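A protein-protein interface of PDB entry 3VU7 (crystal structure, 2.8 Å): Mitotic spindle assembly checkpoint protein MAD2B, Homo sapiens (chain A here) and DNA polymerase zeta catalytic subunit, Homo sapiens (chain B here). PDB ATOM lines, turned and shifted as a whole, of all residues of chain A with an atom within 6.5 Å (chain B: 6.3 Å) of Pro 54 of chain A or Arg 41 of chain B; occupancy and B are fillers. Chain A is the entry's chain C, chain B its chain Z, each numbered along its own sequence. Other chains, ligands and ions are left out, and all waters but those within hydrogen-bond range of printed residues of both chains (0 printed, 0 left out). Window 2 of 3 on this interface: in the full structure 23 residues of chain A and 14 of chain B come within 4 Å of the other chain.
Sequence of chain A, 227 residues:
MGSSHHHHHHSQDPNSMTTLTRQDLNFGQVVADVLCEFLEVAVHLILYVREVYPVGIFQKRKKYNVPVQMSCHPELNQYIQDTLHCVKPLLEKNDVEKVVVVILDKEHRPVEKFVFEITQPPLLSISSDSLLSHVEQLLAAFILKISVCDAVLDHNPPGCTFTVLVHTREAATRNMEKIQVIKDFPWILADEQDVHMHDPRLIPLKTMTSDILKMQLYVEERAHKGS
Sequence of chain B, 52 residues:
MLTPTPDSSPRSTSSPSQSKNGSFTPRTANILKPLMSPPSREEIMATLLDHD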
ATOM      1  N   LEU A  47      12.819 -21.633  27.314  1.00  0.00           N
ATOM      2  CA  LEU A  47      11.404 -21.315  27.525  1.00  0.00           C
ATOM      3  C   LEU A  47      11.200 -20.843  28.953  1.00  0.00           C
ATOM      4  O   LEU A  47      10.395 -19.977  29.231  1.00  0.00           O
ATOM      5  CB  LEU A  47      10.542 -22.536  27.225  1.00  0.00           C
ATOM      6  CG  LEU A  47      10.603 -23.119  25.805  1.00  0.00           C
ATOM      7  CD1 LEU A  47       9.731 -24.361  25.752  1.00  0.00           C
ATOM      8  CD2 LEU A  47      10.169 -22.082  24.774  1.00  0.00           C
ATOM      9  N   TYR A  48      11.972 -21.395  29.868  1.00  0.00           N
ATOM     10  CA  TYR A  48      11.936 -20.910  31.229  1.00  0.00           C
ATOM     11  C   TYR A  48      12.540 -19.513  31.363  1.00  0.00           C
ATOM     12  O   TYR A  48      11.884 -18.633  31.862  1.00  0.00           O
ATOM     13  CB  TYR A  48      12.647 -21.880  32.161  1.00  0.00           C
ATOM     14  CG  TYR A  48      12.819 -21.393  33.589  1.00  0.00           C
ATOM     15  CD1 TYR A  48      11.793 -21.524  34.517  1.00  0.00           C
ATOM     16  CD2 TYR A  48      14.033 -20.848  34.022  1.00  0.00           C
ATOM     17  CE1 TYR A  48      11.956 -21.112  35.829  1.00  0.00           C
ATOM     18  CE2 TYR A  48      14.214 -20.432  35.333  1.00  0.00           C
ATOM     19  CZ  TYR A  48      13.167 -20.562  36.233  1.00  0.00           C
ATOM     20  OH  TYR A  48      13.313 -20.138  37.539  1.00  0.00           O
ATOM     21  N   ARG A  50      13.340 -17.189  29.187  1.00  0.00           N
ATOM     22  CA  ARG A  50      12.625 -16.176  28.426  1.00  0.00           C
ATOM     23  C   ARG A  50      11.176 -16.037  28.852  1.00  0.00           C
ATOM     24  O   ARG A  50      10.457 -15.221  28.295  1.00  0.00           O
ATOM     25  CB  ARG A  50      12.677 -16.481  26.926  1.00  0.00           C
ATOM     26  CG  ARG A  50      14.066 -16.409  26.324  1.00  0.00           C
ATOM     27  CD  ARG A  50      14.867 -15.285  26.948  1.00  0.00           C
ATOM     28  NE  ARG A  50      14.644 -14.012  26.266  1.00  0.00           N
ATOM     29  CZ  ARG A  50      14.920 -12.835  26.799  1.00  0.00           C
ATOM     30  NH1 ARG A  50      15.396 -12.752  28.032  1.00  0.00           N
ATOM     31  NH2 ARG A  50      14.715 -11.747  26.093  1.00  0.00           N
ATOM     32  N   GLU A  51      10.730 -16.860  29.796  1.00  0.00           N
ATOM     33  CA  GLU A  51       9.373 -16.764  30.354  1.00  0.00           C
ATOM     34  C   GLU A  51       8.271 -16.948  29.293  1.00  0.00           C
ATOM     35  O   GLU A  51       7.268 -16.248  29.280  1.00  0.00           O
ATOM     36  CB  GLU A  51       9.201 -15.458  31.139  1.00  0.00           C
ATOM     37  CG  GLU A  51      10.395 -15.056  31.999  1.00  0.00           C
ATOM     38  CD  GLU A  51      10.060 -13.960  33.014  1.00  0.00           C
ATOM     39  OE1 GLU A  51      10.205 -14.190  34.232  1.00  0.00           O
ATOM     40  OE2 GLU A  51       9.652 -12.853  32.616  1.00  0.00           O
ATOM     41  N   VAL A  52       8.477 -17.902  28.398  1.00  0.00           N
ATOM     42  CA  VAL A  52       7.507 -18.242  27.356  1.00  0.00           C
ATOM     43  C   VAL A  52       6.393 -19.116  27.944  1.00  0.00           C
ATOM     44  O   VAL A  52       5.321 -19.297  27.342  1.00  0.00           O
ATOM     45  CB  VAL A  52       8.198 -18.987  26.210  1.00  0.00           C
ATOM     46  CG1 VAL A  52       7.203 -19.326  25.108  1.00  0.00           C
ATOM     47  CG2 VAL A  52       9.381 -18.162  25.673  1.00  0.00           C
ATOM     48  N   TYR A  53       6.673 -19.658  29.127  1.00  0.00           N
ATOM     49  CA  TYR A  53       5.720 -20.401  29.918  1.00  0.00           C
ATOM     50  C   TYR A  53       5.951 -20.043  31.374  1.00  0.00           C
ATOM     51  O   TYR A  53       7.088 -19.808  31.796  1.00  0.00           O
ATOM     52  CB  TYR A  53       5.900 -21.921  29.710  1.00  0.00           C
ATOM     53  CG  TYR A  53       5.447 -22.355  28.348  1.00  0.00           C
ATOM     54  CD1 TYR A  53       4.092 -22.450  28.056  1.00  0.00           C
ATOM     55  CD2 TYR A  53       6.358 -22.576  27.334  1.00  0.00           C
ATOM     56  CE1 TYR A  53       3.653 -22.794  26.810  1.00  0.00           C
ATOM     57  CE2 TYR A  53       5.925 -22.929  26.074  1.00  0.00           C
ATOM     58  CZ  TYR A  53       4.564 -23.028  25.821  1.00  0.00           C
ATOM     59  OH  TYR A  53       4.106 -23.389  24.574  1.00  0.00           O
ATOM     60  N   PRO A  54       4.868 -20.008  32.149  1.00  0.00           N
ATOM     61  CA  PRO A  54       4.824 -19.595  33.543  1.00  0.00           C
ATOM     62  C   PRO A  54       5.743 -20.444  34.384  1.00  0.00           C
ATOM     63  O   PRO A  54       5.836 -21.658  34.162  1.00  0.00           O
ATOM     64  CB  PRO A  54       3.383 -19.882  33.969  1.00  0.00           C
ATOM     65  CG  PRO A  54       2.608 -20.113  32.727  1.00  0.00           C
ATOM     66  CD  PRO A  54       3.571 -20.504  31.661  1.00  0.00           C
ATOM     67  N   VAL A  55       6.378 -19.809  35.369  1.00  0.00           N
ATOM     68  CA  VAL A  55       7.385 -20.460  36.207  1.00  0.00           C
ATOM     69  C   VAL A  55       6.962 -21.855  36.683  1.00  0.00           C
ATOM     70  O   VAL A  55       7.791 -22.750  36.851  1.00  0.00           O
ATOM     71  CB  VAL A  55       7.737 -19.576  37.422  1.00  0.00           C
ATOM     72  CG1 VAL A  55       6.608 -19.572  38.463  1.00  0.00           C
ATOM     73  CG2 VAL A  55       9.072 -20.003  38.026  1.00  0.00           C
ATOM     74  N   GLY A  56       5.654 -22.020  36.862  1.00  0.00           N
ATOM     75  CA  GLY A  56       5.110 -23.099  37.653  1.00  0.00           C
ATOM     76  C   GLY A  56       5.032 -24.478  37.039  1.00  0.00           C
ATOM     77  O   GLY A  56       4.795 -25.436  37.763  1.00  0.00           O
ATOM     78  N   ILE A  57       5.212 -24.596  35.721  1.00  0.00           N
ATOM     79  CA  ILE A  57       5.222 -25.919  35.057  1.00  0.00           C
ATOM     80  C   ILE A  57       6.639 -26.464  34.951  1.00  0.00           C
ATOM     81  O   ILE A  57       6.862 -27.571  34.428  1.00  0.00           O
ATOM     82  CB  ILE A  57       4.589 -25.916  33.641  1.00  0.00           C
ATOM     83  CG1 ILE A  57       5.354 -24.978  32.724  1.00  0.00           C
ATOM     84  CG2 ILE A  57       3.113 -25.557  33.687  1.00  0.00           C
ATOM     85  CD1 ILE A  57       5.562 -25.599  31.380  1.00  0.00           C
ATOM     86  N   PHE A  58       7.598 -25.688  35.440  1.00  0.00           N
ATOM     87  CA  PHE A  58       8.965 -26.126  35.369  1.00  0.00           C
ATOM     88  C   PHE A  58       9.365 -26.719  36.682  1.00  0.00           C
ATOM     89  O   PHE A  58       8.927 -26.267  37.716  1.00  0.00           O
ATOM     90  CB  PHE A  58       9.892 -24.980  34.984  1.00  0.00           C
ATOM     91  CG  PHE A  58       9.712 -24.505  33.559  1.00  0.00           C
ATOM     92  CD1 PHE A  58      10.456 -25.060  32.521  1.00  0.00           C
ATOM     93  CD2 PHE A  58       8.789 -23.494  33.266  1.00  0.00           C
ATOM     94  CE1 PHE A  58      10.285 -24.604  31.222  1.00  0.00           C
ATOM     95  CE2 PHE A  58       8.620 -23.029  31.972  1.00  0.00           C
ATOM     96  CZ  PHE A  58       9.373 -23.583  30.949  1.00  0.00           C
ATOM     97  N   GLY A 159       2.981 -12.299  26.058  1.00  0.00           N
ATOM     98  CA  GLY A 159       2.217 -13.127  25.125  1.00  0.00           C
ATOM     99  C   GLY A 159       3.023 -13.707  23.982  1.00  0.00           C
ATOM    100  O   GLY A 159       2.505 -13.892  22.876  1.00  0.00           O
ATOM    101  N   CYS A 160       4.298 -13.978  24.241  1.00  0.00           N
ATOM    102  CA  CYS A 160       5.173 -14.613  23.251  1.00  0.00           C
ATOM    103  C   CYS A 160       4.970 -16.113  23.171  1.00  0.00           C
ATOM    104  O   CYS A 160       4.843 -16.821  24.178  1.00  0.00           O
ATOM    105  CB  CYS A 160       6.651 -14.317  23.536  1.00  0.00           C
ATOM    106  SG  CYS A 160       7.148 -12.644  23.064  1.00  0.00           S
ATOM    107  N   PRO B  39       1.871 -26.039  22.560  1.00  0.00           N
ATOM    108  CA  PRO B  39       0.673 -25.767  23.351  1.00  0.00           C
ATOM    109  C   PRO B  39       0.700 -24.330  23.830  1.00  0.00           C
ATOM    110  O   PRO B  39       1.756 -23.852  24.249  1.00  0.00           O
ATOM    111  CB  PRO B  39       0.837 -26.692  24.562  1.00  0.00           C
ATOM    112  CG  PRO B  39       1.847 -27.701  24.157  1.00  0.00           C
ATOM    113  CD  PRO B  39       2.782 -26.944  23.276  1.00  0.00           C
ATOM    114  N   SER B  40      -0.446 -23.650  23.766  1.00  0.00           N
ATOM    115  CA  SER B  40      -0.524 -22.236  24.123  1.00  0.00           C
ATOM    116  C   SER B  40      -0.371 -22.028  25.620  1.00  0.00           C
ATOM    117  O   SER B  40      -0.696 -22.917  26.392  1.00  0.00           O
ATOM    118  CB  SER B  40      -1.859 -21.690  23.662  1.00  0.00           C
ATOM    119  OG  SER B  40      -2.907 -22.424  24.263  1.00  0.00           O
ATOM    120  N   ARG B  41       0.118 -20.855  26.026  1.00  0.00           N
ATOM    121  CA  ARG B  41       0.192 -20.489  27.448  1.00  0.00           C
ATOM    122  C   ARG B  41      -1.091 -20.828  28.201  1.00  0.00           C
ATOM    123  O   ARG B  41      -1.042 -21.262  29.344  1.00  0.00           O
ATOM    124  CB  ARG B  41       0.457 -19.005  27.631  1.00  0.00           C
ATOM    125  CG  ARG B  41       1.875 -18.577  27.377  1.00  0.00           C
ATOM    126  CD  ARG B  41       2.083 -17.152  27.845  1.00  0.00           C
ATOM    127  NE  ARG B  41       2.264 -17.086  29.294  1.00  0.00           N
ATOM    128  CZ  ARG B  41       3.451 -17.013  29.904  1.00  0.00           C
ATOM    129  NH1 ARG B  41       4.583 -16.999  29.201  1.00  0.00           N
ATOM    130  NH2 ARG B  41       3.516 -16.956  31.228  1.00  0.00           N
ATOM    131  N   GLU B  42      -2.234 -20.631  27.556  1.00  0.00           N
ATOM    132  CA  GLU B  42      -3.537 -20.889  28.160  1.00  0.00           C
ATOM    133  C   GLU B  42      -3.763 -22.363  28.514  1.00  0.00           C
ATOM    134  O   GLU B  42      -4.079 -22.681  29.656  1.00  0.00           O
ATOM    135  CB  GLU B  42      -4.639 -20.369  27.238  1.00  0.00           C
ATOM    136  CG  GLU B  42      -4.675 -18.849  27.098  1.00  0.00           C
ATOM    137  CD  GLU B  42      -3.314 -18.222  26.824  1.00  0.00           C
ATOM    138  OE1 GLU B  42      -2.603 -18.690  25.902  1.00  0.00           O
ATOM    139  OE2 GLU B  42      -2.952 -17.255  27.535  1.00  0.00           O
ATOM    140  N   GLU B  43      -3.579 -23.257  27.546  1.00  0.00           N
ATOM    141  CA  GLU B  43      -3.775 -24.694  27.759  1.00  0.00           C
ATOM    142  C   GLU B  43      -2.883 -25.275  28.858  1.00  0.00           C
ATOM    143  O   GLU B  43      -3.159 -26.344  29.400  1.00  0.00           O
ATOM    144  CB  GLU B  43      -3.550 -25.459  26.458  1.00  0.00           C
ATOM    145  CG  GLU B  43      -4.165 -26.851  26.469  1.00  0.00           C
ATOM    146  CD  GLU B  43      -3.752 -27.702  25.285  1.00  0.00           C
ATOM    147  OE1 GLU B  43      -4.625 -28.416  24.747  1.00  0.00           O
ATOM    148  OE2 GLU B  43      -2.566 -27.668  24.894  1.00  0.00           O
ATOM    149  N   ILE B  44      -1.810 -24.564  29.170  1.00  0.00           N
ATOM    150  CA  ILE B  44      -0.910 -24.938  30.242  1.00  0.00           C
ATOM    151  C   ILE B  44      -1.541 -24.486  31.540  1.00  0.00           C
ATOM    152  O   ILE B  44      -1.732 -25.284  32.462  1.00  0.00           O
ATOM    153  CB  ILE B  44       0.461 -24.238  30.096  1.00  0.00           C
ATOM    154  CG1 ILE B  44       1.161 -24.620  28.778  1.00  0.00           C
ATOM    155  CG2 ILE B  44       1.342 -24.464  31.317  1.00  0.00           C
ATOM    156  CD1 ILE B  44       1.654 -26.045  28.663  1.00  0.00           C
ATOM    157  N   MET B  45      -1.861 -23.194  31.604  1.00  0.00           N
ATOM    158  CA  MET B  45      -2.548 -22.626  32.756  1.00  0.00           C
ATOM    159  C   MET B  45      -3.840 -23.395  33.027  1.00  0.00           C
ATOM    160  O   MET B  45      -4.406 -23.280  34.111  1.00  0.00           O
ATOM    161  CB  MET B  45      -2.811 -21.124  32.573  1.00  0.00           C
ATOM    162  CG  MET B  45      -1.550 -20.264  32.553  1.00  0.00           C
ATOM    163  SD  MET B  45      -1.796 -18.473  32.627  1.00  0.00           S
ATOM    164  CE  MET B  45      -2.930 -18.161  31.258  1.00  0.00           C
ATOM    165  N   ALA B  46      -4.288 -24.184  32.047  1.00  0.00           N
ATOM    166  CA  ALA B  46      -5.284 -25.220  32.289  1.00  0.00           C
ATOM    167  C   ALA B  46      -4.693 -26.247  33.256  1.00  0.00           C
ATOM    168  O   ALA B  46      -4.913 -27.451  33.110  1.00  0.00           O
ATOM    169  CB  ALA B  46      -5.715 -25.876  30.991  1.00  0.00           C
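The backbone carbonyl oxygen (O) of Glu 51 of chain A sits at hydrogen-bond distance from the guanidinium group (NH1) of Arg 41 of chain B, 2.8 Å away.
The guanidinium group of Arg 41 of chain B is in hydrogen-bond range of the backbone carbonyl oxygen of Val 52 of chain A, at 3.0 Å.
O of Pro 39 of chain B is in hydrogen-bond range of OH of Tyr 53 of chain A, 2.4 Å away.
NH1 of Arg 41 of chain B lies close to N of Tyr 53 of chain A (3.4 Å).
N of Pro 54 of chain A lies close to NH2 of Arg 41 of chain B, at 3.5 Å.
Of the 13 printed residues of chain A, 5 touch a printed residue of chain B.
Printed residues of chain A that touch a printed residue of chain B: Glu 51, Val 52, Tyr 53, Pro 54 and Ile 57.
Hydrophobic or aromatic side chains of chain B within 4 Å of the printed part of chain A: Ile 44.
Among the printed residues, no Asp or Glu carboxylate lies within 4 Å of a Lys or Arg side-chain nitrogen of the other chain.
Of chain B, only Arg 41 (3.5 Å) comes within 4 Å of Pro 54 of chain A.
Of chain A, only Glu 51, Val 52, Tyr 53 and Pro 54 come within 4 Å of Arg 41 of chain B.
Of the printed residues of chain B, Tyr 53 of chain A touches Pro 39 (2.4 Å), Arg 41 (3.4 Å) and Ile 44 (3.7 Å).
Of the printed residues of chain B, Glu 51 of chain A touches Arg 41.
Of the printed residues of chain B, Val 52 of chain A touches Arg 41 (3.0 Å).
The nearest printed residue of chain B that does not touch Tyr 53 of chain A is Ser 40 of chain B (4.3 Å).
CE1 of Tyr 53 of chain A touches CG1 of Ile 44 of chain B (3.7 Å).
Ile 44 of chain B touches Ile 57 of chain A.
The backbone NH of Val 52 of chain A is in hydrogen-bond range of the backbone carbonyl oxygen of Leu 47 of chain A, 2.9 Å away.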
